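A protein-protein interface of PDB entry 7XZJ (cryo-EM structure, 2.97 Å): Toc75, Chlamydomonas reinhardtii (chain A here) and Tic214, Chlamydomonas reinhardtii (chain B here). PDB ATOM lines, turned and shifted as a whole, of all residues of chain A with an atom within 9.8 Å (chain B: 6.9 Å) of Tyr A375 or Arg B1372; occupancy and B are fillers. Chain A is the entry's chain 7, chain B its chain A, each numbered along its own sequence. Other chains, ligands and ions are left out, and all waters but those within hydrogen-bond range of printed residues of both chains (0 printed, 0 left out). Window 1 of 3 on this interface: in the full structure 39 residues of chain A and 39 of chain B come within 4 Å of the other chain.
The side-chain hydroxyl (OH) of Tyr A375 is in hydrogen-bond range of the side-chain carboxylate (OD2) of Asp B1386, at 2.9 Å. The side-chain amide nitrogen (ND2) of Asn A379 lies within hydrogen-bond range of the backbone carbonyl oxygen (O) of Arg B1372, at 2.9 Å.
The backbone carbonyl oxygen of Tyr A375 lies close to the side-chain amide oxygen of Asn A379 (3.2 Å). The backbone carbonyl oxygen (O) of Ala B1370 lies within hydrogen-bond range of the guanidinium group (NH1) of Arg B1372. NH2 of Arg B1372 lies within salt-bridge range of OD1 of Asp B1386.
Among the printed residues, pairs that only touch across the chains: Glu A372 with Ile B1385 (3.2 Å), Tyr A375 with Arg B1372 (3.5 Å), Asp A376 with Ile B1385 (3.1 Å), Met A378 with Thr B1369 (3.7 Å), Met A378 with Ala B1370 (3.7 Å), Asn A379 with Thr B1371 (3.5 Å) and Phe A382 with Thr B1371 (3.6 Å).
Val A371 touches none of the printed residues of chain B. Of chain B, only Arg B1372 and Asp B1386 come within 4 Å of Tyr A375. Of the printed residues of chain B, Phe A382 touches Thr B1371. Printed residues of chain A within 4 Å of Thr B1369: Met A378 (3.7 Å). Of the printed residues of chain A, Ala B1370 touches Met A378 (3.7 Å). Of chain A, only Asn A379 (3.5 Å) and Phe A382 (3.6 Å) come within 4 Å of Thr B1371. Of chain A, only Tyr A375 and Asn A379 come within 4 Å of Arg B1372. The nearest printed residue of chain B that does not touch Asn A379 is Pro B1374 (4.6 Å).
Printed residues of chain B that touch a printed residue of chain A: Thr B1369, Ala B1370, Thr B1371, Arg B1372, Ile B1385 and Asp B1386. Hydrophobic or aromatic side chains of chain B that line the printed part of chain A: Ile B1385. Among the printed residues, 9 pairs touch across the chains. Among the printed residues, no Asp or Glu carboxylate lies within 4 Å of a Lys or Arg side-chain nitrogen of the other chain.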
ATOM      1  N   GLY A 297       8.426  38.114  23.344  1.00  0.00           N
ATOM      2  CA  GLY A 297       8.718  36.916  24.100  1.00  0.00           C
ATOM      3  C   GLY A 297       9.312  37.126  25.474  1.00  0.00           C
ATOM      4  O   GLY A 297       9.684  36.141  26.121  1.00  0.00           O
ATOM      5  N   PRO A 299       8.529  37.840  29.215  1.00  0.00           N
ATOM      6  CA  PRO A 299       7.360  37.933  30.089  1.00  0.00           C
ATOM      7  C   PRO A 299       7.648  38.603  31.440  1.00  0.00           C
ATOM      8  O   PRO A 299       6.713  38.805  32.187  1.00  0.00           O
ATOM      9  CB  PRO A 299       7.031  36.453  30.318  1.00  0.00           C
ATOM     10  CG  PRO A 299       8.385  35.789  30.415  1.00  0.00           C
ATOM     11  CD  PRO A 299       9.302  36.614  29.536  1.00  0.00           C
ATOM     12  N   ALA A 360      26.259  24.315  31.121  1.00  0.00           N
ATOM     13  CA  ALA A 360      25.484  23.789  29.972  1.00  0.00           C
ATOM     14  C   ALA A 360      24.158  24.541  29.822  1.00  0.00           C
ATOM     15  O   ALA A 360      23.577  24.488  28.725  1.00  0.00           O
ATOM     16  CB  ALA A 360      25.257  22.309  30.146  1.00  0.00           C
ATOM     17  N   SER A 361      23.693  25.196  30.887  1.00  0.00           N
ATOM     18  CA  SER A 361      22.459  25.969  30.792  1.00  0.00           C
ATOM     19  C   SER A 361      22.622  27.168  29.870  1.00  0.00           C
ATOM     20  O   SER A 361      21.702  27.508  29.117  1.00  0.00           O
ATOM     21  CB  SER A 361      22.018  26.423  32.183  1.00  0.00           C
ATOM     22  OG  SER A 361      23.005  27.244  32.781  1.00  0.00           O
ATOM     23  N   PHE A 363      23.098  30.331  31.051  1.00  0.00           N
ATOM     24  CA  PHE A 363      22.381  31.473  31.681  1.00  0.00           C
ATOM     25  C   PHE A 363      23.404  32.495  32.183  1.00  0.00           C
ATOM     26  O   PHE A 363      24.219  32.144  33.058  1.00  0.00           O
ATOM     27  CB  PHE A 363      21.440  30.986  32.786  1.00  0.00           C
ATOM     28  CG  PHE A 363      20.086  30.541  32.295  1.00  0.00           C
ATOM     29  CD1 PHE A 363      19.393  31.288  31.357  1.00  0.00           C
ATOM     30  CD2 PHE A 363      19.497  29.382  32.777  1.00  0.00           C
ATOM     31  CE1 PHE A 363      18.146  30.883  30.905  1.00  0.00           C
ATOM     32  CE2 PHE A 363      18.250  28.979  32.325  1.00  0.00           C
ATOM     33  CZ  PHE A 363      17.577  29.730  31.391  1.00  0.00           C
ATOM     34  N   TYR A 369      15.749  37.903  30.549  1.00  0.00           N
ATOM     35  CA  TYR A 369      15.244  36.509  30.443  1.00  0.00           C
ATOM     36  C   TYR A 369      14.389  36.332  29.187  1.00  0.00           C
ATOM     37  O   TYR A 369      13.627  37.252  28.841  1.00  0.00           O
ATOM     38  CB  TYR A 369      14.457  36.103  31.690  1.00  0.00           C
ATOM     39  CG  TYR A 369      13.859  34.720  31.611  1.00  0.00           C
ATOM     40  CD1 TYR A 369      12.526  34.532  31.282  1.00  0.00           C
ATOM     41  CD2 TYR A 369      14.633  33.594  31.838  1.00  0.00           C
ATOM     42  CE1 TYR A 369      11.976  33.265  31.191  1.00  0.00           C
ATOM     43  CE2 TYR A 369      14.099  32.320  31.752  1.00  0.00           C
ATOM     44  CZ  TYR A 369      12.765  32.155  31.428  1.00  0.00           C
ATOM     45  OH  TYR A 369      12.230  30.902  31.344  1.00  0.00           O
ATOM     46  N   HIS A 370      14.505  35.172  28.540  1.00  0.00           N
ATOM     47  CA  HIS A 370      13.668  34.861  27.354  1.00  0.00           C
ATOM     48  C   HIS A 370      13.258  33.391  27.477  1.00  0.00           C
ATOM     49  O   HIS A 370      14.086  32.597  27.953  1.00  0.00           O
ATOM     50  CB  HIS A 370      14.449  35.177  26.072  1.00  0.00           C
ATOM     51  CG  HIS A 370      13.627  35.193  24.829  1.00  0.00           C
ATOM     52  ND1 HIS A 370      12.248  35.168  24.850  1.00  0.00           N
ATOM     53  CD2 HIS A 370      13.984  35.247  23.529  1.00  0.00           C
ATOM     54  CE1 HIS A 370      11.792  35.195  23.614  1.00  0.00           C
ATOM     55  NE2 HIS A 370      12.837  35.245  22.786  1.00  0.00           N
ATOM     56  N   VAL A 371      12.022  33.050  27.111  1.00  0.00           N
ATOM     57  CA  VAL A 371      11.523  31.660  27.247  1.00  0.00           C
ATOM     58  C   VAL A 371      12.304  30.770  26.286  1.00  0.00           C
ATOM     59  O   VAL A 371      12.878  29.786  26.716  1.00  0.00           O
ATOM     60  CB  VAL A 371      10.017  31.628  26.966  1.00  0.00           C
ATOM     61  CG1 VAL A 371       9.224  32.134  28.156  1.00  0.00           C
ATOM     62  CG2 VAL A 371       9.662  32.405  25.709  1.00  0.00           C
ATOM     63  N   GLU A 372      12.388  31.167  25.014  1.00  0.00           N
ATOM     64  CA  GLU A 372      13.130  30.377  23.998  1.00  0.00           C
ATOM     65  C   GLU A 372      14.495  29.987  24.568  1.00  0.00           C
ATOM     66  O   GLU A 372      14.976  28.896  24.230  1.00  0.00           O
ATOM     67  CB  GLU A 372      13.261  31.183  22.707  1.00  0.00           C
ATOM     68  CG  GLU A 372      11.973  31.860  22.273  1.00  0.00           C
ATOM     69  CD  GLU A 372      10.931  30.980  21.605  1.00  0.00           C
ATOM     70  OE1 GLU A 372      10.524  29.969  22.213  1.00  0.00           O
ATOM     71  OE2 GLU A 372      10.524  31.309  20.474  1.00  0.00           O
ATOM     72  N   ASP A 373      15.077  30.837  25.418  1.00  0.00           N
ATOM     73  CA  ASP A 373      16.379  30.516  26.063  1.00  0.00           C
ATOM     74  C   ASP A 373      16.206  29.274  26.941  1.00  0.00           C
ATOM     75  O   ASP A 373      17.146  28.466  26.993  1.00  0.00           O
ATOM     76  CB  ASP A 373      16.939  31.712  26.832  1.00  0.00           C
ATOM     77  CG  ASP A 373      17.608  32.732  25.934  1.00  0.00           C
ATOM     78  OD1 ASP A 373      18.086  32.334  24.855  1.00  0.00           O
ATOM     79  OD2 ASP A 373      17.639  33.917  26.316  1.00  0.00           O
ATOM     80  N   GLY A 374      15.107  29.202  27.697  1.00  0.00           N
ATOM     81  CA  GLY A 374      14.854  28.056  28.592  1.00  0.00           C
ATOM     82  C   GLY A 374      14.586  26.786  27.808  1.00  0.00           C
ATOM     83  O   GLY A 374      14.996  25.715  28.281  1.00  0.00           O
ATOM     84  N   TYR A 375      13.909  26.892  26.661  1.00  0.00           N
ATOM     85  CA  TYR A 375      13.699  25.696  25.803  1.00  0.00           C
ATOM     86  C   TYR A 375      15.060  25.198  25.312  1.00  0.00           C
ATOM     87  O   TYR A 375      15.278  23.976  25.311  1.00  0.00           O
ATOM     88  CB  TYR A 375      12.753  26.015  24.642  1.00  0.00           C
ATOM     89  CG  TYR A 375      11.379  26.466  25.065  1.00  0.00           C
ATOM     90  CD1 TYR A 375      10.611  25.703  25.927  1.00  0.00           C
ATOM     91  CD2 TYR A 375      10.842  27.652  24.598  1.00  0.00           C
ATOM     92  CE1 TYR A 375       9.348  26.111  26.323  1.00  0.00           C
ATOM     93  CE2 TYR A 375       9.581  28.076  24.981  1.00  0.00           C
ATOM     94  CZ  TYR A 375       8.830  27.301  25.847  1.00  0.00           C
ATOM     95  OH  TYR A 375       7.585  27.709  26.229  1.00  0.00           O
ATOM     96  N   ASP A 376      15.947  26.121  24.927  1.00  0.00           N
ATOM     97  CA  ASP A 376      17.315  25.731  24.496  1.00  0.00           C
ATOM     98  C   ASP A 376      18.057  25.168  25.707  1.00  0.00           C
ATOM     99  O   ASP A 376      18.770  24.160  25.548  1.00  0.00           O
ATOM    100  CB  ASP A 376      18.084  26.927  23.933  1.00  0.00           C
ATOM    101  CG  ASP A 376      17.448  27.535  22.697  1.00  0.00           C
ATOM    102  OD1 ASP A 376      16.779  26.790  21.956  1.00  0.00           O
ATOM    103  OD2 ASP A 376      17.620  28.752  22.492  1.00  0.00           O
ATOM    104  N   ALA A 377      17.895  25.807  26.868  1.00  0.00           N
ATOM    105  CA  ALA A 377      18.583  25.350  28.096  1.00  0.00           C
ATOM    106  C   ALA A 377      18.118  23.932  28.431  1.00  0.00           C
ATOM    107  O   ALA A 377      18.963  23.119  28.835  1.00  0.00           O
ATOM    108  CB  ALA A 377      18.315  26.304  29.230  1.00  0.00           C
ATOM    109  N   MET A 378      16.822  23.657  28.267  1.00  0.00           N
ATOM    110  CA  MET A 378      16.276  22.302  28.546  1.00  0.00           C
ATOM    111  C   MET A 378      16.911  21.294  27.585  1.00  0.00           C
ATOM    112  O   MET A 378      17.333  20.227  28.057  1.00  0.00           O
ATOM    113  CB  MET A 378      14.756  22.292  28.356  1.00  0.00           C
ATOM    114  CG  MET A 378      14.140  20.907  28.279  1.00  0.00           C
ATOM    115  SD  MET A 378      14.107  20.043  29.868  1.00  0.00           S
ATOM    116  CE  MET A 378      13.267  18.533  29.396  1.00  0.00           C
ATOM    117  N   ASN A 379      17.025  21.643  26.301  1.00  0.00           N
ATOM    118  CA  ASN A 379      17.546  20.669  25.308  1.00  0.00           C
ATOM    119  C   ASN A 379      18.990  20.302  25.661  1.00  0.00           C
ATOM    120  O   ASN A 379      19.311  19.101  25.634  1.00  0.00           O
ATOM    121  CB  ASN A 379      17.465  21.222  23.887  1.00  0.00           C
ATOM    122  CG  ASN A 379      16.052  21.556  23.461  1.00  0.00           C
ATOM    123  OD1 ASN A 379      15.091  21.070  24.049  1.00  0.00           O
ATOM    124  ND2 ASN A 379      15.921  22.391  22.444  1.00  0.00           N
ATOM    125  N   SER A 380      19.818  21.296  25.990  1.00  0.00           N
ATOM    126  CA  SER A 380      21.248  21.030  26.296  1.00  0.00           C
ATOM    127  C   SER A 380      21.386  20.194  27.572  1.00  0.00           C
ATOM    128  O   SER A 380      22.199  19.254  27.569  1.00  0.00           O
ATOM    129  CB  SER A 380      22.021  22.315  26.395  1.00  0.00           C
ATOM    130  OG  SER A 380      23.382  22.062  26.709  1.00  0.00           O
ATOM    131  N   ILE A 381      20.646  20.543  28.627  1.00  0.00           N
ATOM    132  CA  ILE A 381      20.765  19.825  29.931  1.00  0.00           C
ATOM    133  C   ILE A 381      20.264  18.390  29.751  1.00  0.00           C
ATOM    134  O   ILE A 381      20.935  17.466  30.247  1.00  0.00           O
ATOM    135  CB  ILE A 381      19.988  20.570  31.033  1.00  0.00           C
ATOM    136  CG1 ILE A 381      20.614  21.932  31.339  1.00  0.00           C
ATOM    137  CG2 ILE A 381      19.873  19.722  32.291  1.00  0.00           C
ATOM    138  CD1 ILE A 381      22.022  21.844  31.866  1.00  0.00           C
ATOM    139  N   PHE A 382      19.151  18.215  29.035  1.00  0.00           N
ATOM    140  CA  PHE A 382      18.547  16.867  28.857  1.00  0.00           C
ATOM    141  C   PHE A 382      19.511  15.941  28.107  1.00  0.00           C
ATOM    142  O   PHE A 382      19.503  14.741  28.411  1.00  0.00           O
ATOM    143  CB  PHE A 382      17.189  16.962  28.158  1.00  0.00           C
ATOM    144  CG  PHE A 382      16.203  15.901  28.575  1.00  0.00           C
ATOM    145  CD1 PHE A 382      15.838  15.756  29.904  1.00  0.00           C
ATOM    146  CD2 PHE A 382      15.633  15.051  27.641  1.00  0.00           C
ATOM    147  CE1 PHE A 382      14.930  14.782  30.290  1.00  0.00           C
ATOM    148  CE2 PHE A 382      14.724  14.078  28.028  1.00  0.00           C
ATOM    149  CZ  PHE A 382      14.375  13.945  29.352  1.00  0.00           C
ATOM    150  N   ALA A 383      20.254  16.470  27.129  1.00  0.00           N
ATOM    151  CA  ALA A 383      21.183  15.649  26.316  1.00  0.00           C
ATOM    152  C   ALA A 383      22.005  14.691  27.192  1.00  0.00           C
ATOM    153  O   ALA A 383      22.404  13.637  26.674  1.00  0.00           O
ATOM    154  CB  ALA A 383      22.066  16.536  25.475  1.00  0.00           C
ATOM    155  N   ILE A 392      13.036  23.848  35.485  1.00  0.00           N
ATOM    156  CA  ILE A 392      13.688  25.149  35.573  1.00  0.00           C
ATOM    157  C   ILE A 392      12.613  26.215  35.727  1.00  0.00           C
ATOM    158  O   ILE A 392      11.662  26.263  34.939  1.00  0.00           O
ATOM    159  CB  ILE A 392      14.571  25.425  34.342  1.00  0.00           C
ATOM    160  CG1 ILE A 392      14.900  26.916  34.236  1.00  0.00           C
ATOM    161  CG2 ILE A 392      13.902  24.911  33.072  1.00  0.00           C
ATOM    162  N   PRO A 394      12.123  30.464  36.623  1.00  0.00           N
ATOM    163  CA  PRO A 394      12.547  31.811  37.028  1.00  0.00           C
ATOM    164  C   PRO A 394      11.534  32.434  37.982  1.00  0.00           C
ATOM    165  O   PRO A 394      10.330  32.439  37.712  1.00  0.00           O
ATOM    166  CB  PRO A 394      12.610  32.573  35.701  1.00  0.00           C
ATOM    167  CG  PRO A 394      11.573  31.912  34.858  1.00  0.00           C
ATOM    168  CD  PRO A 394      11.539  30.453  35.271  1.00  0.00           C
ATOM    169  N   LEU B1368       6.439  18.265  33.521  1.00  0.00           N
ATOM    170  CA  LEU B1368       5.921  19.518  32.911  1.00  0.00           C
ATOM    171  C   LEU B1368       6.802  19.921  31.722  1.00  0.00           C
ATOM    172  O   LEU B1368       6.239  20.324  30.686  1.00  0.00           O
ATOM    173  CB  LEU B1368       5.915  20.608  33.986  1.00  0.00           C
ATOM    174  CG  LEU B1368       5.287  20.204  35.319  1.00  0.00           C
ATOM    175  CD1 LEU B1368       5.507  21.278  36.374  1.00  0.00           C
ATOM    176  CD2 LEU B1368       3.803  19.909  35.159  1.00  0.00           C
ATOM    177  N   THR B1369       8.127  19.812  31.866  1.00  0.00           N
ATOM    178  CA  THR B1369       9.071  20.248  30.799  1.00  0.00           C
ATOM    179  C   THR B1369       9.085  19.263  29.625  1.00  0.00           C
ATOM    180  O   THR B1369       8.867  18.060  29.866  1.00  0.00           O
ATOM    181  CB  THR B1369      10.474  20.463  31.376  1.00  0.00           C
ATOM    182  OG1 THR B1369      10.850  19.258  32.040  1.00  0.00           O
ATOM    183  CG2 THR B1369      10.531  21.626  32.342  1.00  0.00           C
ATOM    184  N   ALA B1370       9.346  19.759  28.410  1.00  0.00           N
ATOM    185  CA  ALA B1370       9.435  18.879  27.220  1.00  0.00           C
ATOM    186  C   ALA B1370      10.626  19.293  26.345  1.00  0.00           C
ATOM    187  O   ALA B1370      10.977  20.488  26.360  1.00  0.00           O
ATOM    188  CB  ALA B1370       8.142  18.925  26.446  1.00  0.00           C
ATOM    189  N   THR B1371      11.191  18.347  25.587  1.00  0.00           N
ATOM    190  CA  THR B1371      12.308  18.665  24.655  1.00  0.00           C
ATOM    191  C   THR B1371      11.725  19.352  23.413  1.00  0.00           C
ATOM    192  O   THR B1371      10.630  18.943  22.983  1.00  0.00           O
ATOM    193  CB  THR B1371      13.093  17.396  24.298  1.00  0.00           C
ATOM    194  OG1 THR B1371      13.262  16.633  25.493  1.00  0.00           O
ATOM    195  CG2 THR B1371      14.444  17.684  23.680  1.00  0.00           C
ATOM    196  N   ARG B1372      12.430  20.346  22.861  1.00  0.00           N
ATOM    197  CA  ARG B1372      11.904  21.116  21.700  1.00  0.00           C
ATOM    198  C   ARG B1372      12.885  21.008  20.529  1.00  0.00           C
ATOM    199  O   ARG B1372      14.099  20.927  20.787  1.00  0.00           O
ATOM    200  CB  ARG B1372      11.747  22.594  22.068  1.00  0.00           C
ATOM    201  CG  ARG B1372      10.722  22.881  23.154  1.00  0.00           C
ATOM    202  CD  ARG B1372       9.316  22.465  22.770  1.00  0.00           C
ATOM    203  NE  ARG B1372       8.302  23.316  23.378  1.00  0.00           N
ATOM    204  CZ  ARG B1372       7.817  23.159  24.604  1.00  0.00           C
ATOM    205  NH1 ARG B1372       8.259  22.179  25.374  1.00  0.00           N
ATOM    206  NH2 ARG B1372       6.896  23.988  25.061  1.00  0.00           N
ATOM    207  N   LYS B1373      12.383  21.032  19.292  1.00  0.00           N
ATOM    208  CA  LYS B1373      13.278  20.980  18.105  1.00  0.00           C
ATOM    209  C   LYS B1373      13.054  22.218  17.233  1.00  0.00           C
ATOM    210  O   LYS B1373      12.004  22.284  16.568  1.00  0.00           O
ATOM    211  CB  LYS B1373      13.026  19.702  17.300  1.00  0.00           C
ATOM    212  CG  LYS B1373      13.903  19.529  16.069  1.00  0.00           C
ATOM    213  CD  LYS B1373      13.478  18.375  15.191  1.00  0.00           C
ATOM    214  CE  LYS B1373      14.260  18.304  13.897  1.00  0.00           C
ATOM    215  NZ  LYS B1373      14.137  19.556  13.116  1.00  0.00           N
ATOM    216  N   PRO B1374      13.983  23.199  17.201  1.00  0.00           N
ATOM    217  CA  PRO B1374      13.833  24.344  16.303  1.00  0.00           C
ATOM    218  C   PRO B1374      13.872  23.839  14.855  1.00  0.00           C
ATOM    219  O   PRO B1374      14.755  23.066  14.529  1.00  0.00           O
ATOM    220  CB  PRO B1374      15.052  25.227  16.611  1.00  0.00           C
ATOM    221  CG  PRO B1374      16.030  24.312  17.323  1.00  0.00           C
ATOM    222  CD  PRO B1374      15.189  23.268  18.025  1.00  0.00           C
ATOM    223  N   ARG B1375      12.925  24.284  14.028  1.00  0.00           N
ATOM    224  CA  ARG B1375      12.853  23.773  12.634  1.00  0.00           C
ATOM    225  C   ARG B1375      12.305  24.861  11.709  1.00  0.00           C
ATOM    226  O   ARG B1375      11.534  25.711  12.193  1.00  0.00           O
ATOM    227  CB  ARG B1375      11.958  22.531  12.594  1.00  0.00           C
ATOM    228  CG  ARG B1375      10.569  22.751  13.178  1.00  0.00           C
ATOM    229  CD  ARG B1375       9.900  21.465  13.623  1.00  0.00           C
ATOM    230  NE  ARG B1375       8.553  21.691  14.129  1.00  0.00           N
ATOM    231  CZ  ARG B1375       8.253  21.945  15.398  1.00  0.00           C
ATOM    232  NH1 ARG B1375       9.210  22.007  16.308  1.00  0.00           N
ATOM    233  NH2 ARG B1375       6.996  22.134  15.754  1.00  0.00           N
ATOM    234  N   ILE B1385      10.323  26.986  17.360  1.00  0.00           N
ATOM    235  CA  ILE B1385      10.871  26.094  18.423  1.00  0.00           C
ATOM    236  C   ILE B1385       9.673  25.742  19.306  1.00  0.00           C
ATOM    237  O   ILE B1385       9.506  24.549  19.632  1.00  0.00           O
ATOM    238  CB  ILE B1385      12.034  26.773  19.177  1.00  0.00           C
ATOM    239  CG1 ILE B1385      12.713  25.817  20.159  1.00  0.00           C
ATOM    240  CG2 ILE B1385      11.576  28.055  19.855  1.00  0.00           C
ATOM    241  CD1 ILE B1385      14.030  26.322  20.689  1.00  0.00           C
ATOM    242  N   ASP B1386       8.856  26.743  19.647  1.00  0.00           N
ATOM    243  CA  ASP B1386       7.590  26.479  20.383  1.00  0.00           C
ATOM    244  C   ASP B1386       6.482  27.272  19.683  1.00  0.00           C
ATOM    245  O   ASP B1386       5.331  26.793  19.675  1.00  0.00           O
ATOM    246  CB  ASP B1386       7.739  26.894  21.848  1.00  0.00           C
ATOM    247  CG  ASP B1386       6.564  26.480  22.716  1.00  0.00           C
ATOM    248  OD1 ASP B1386       5.979  25.415  22.440  1.00  0.00           O
ATOM    249  OD2 ASP B1386       6.238  27.231  23.655  1.00  0.00           O
ATOM    250  N   ASN B1387       6.807  28.461  19.171  1.00  0.00           N
ATOM    251  CA  ASN B1387       5.818  29.287  18.429  1.00  0.00           C
ATOM    252  C   ASN B1387       6.471  29.723  17.118  1.00  0.00           C
ATOM    253  O   ASN B1387       7.707  29.875  17.108  1.00  0.00           O
ATOM    254  CB  ASN B1387       5.373  30.506  19.240  1.00  0.00           C
ATOM    255  CG  ASN B1387       4.526  30.145  20.442  1.00  0.00           C
ATOM    256  OD1 ASN B1387       3.687  29.251  20.371  1.00  0.00           O
ATOM    257  ND2 ASN B1387       4.732  30.842  21.548  1.00  0.00           N
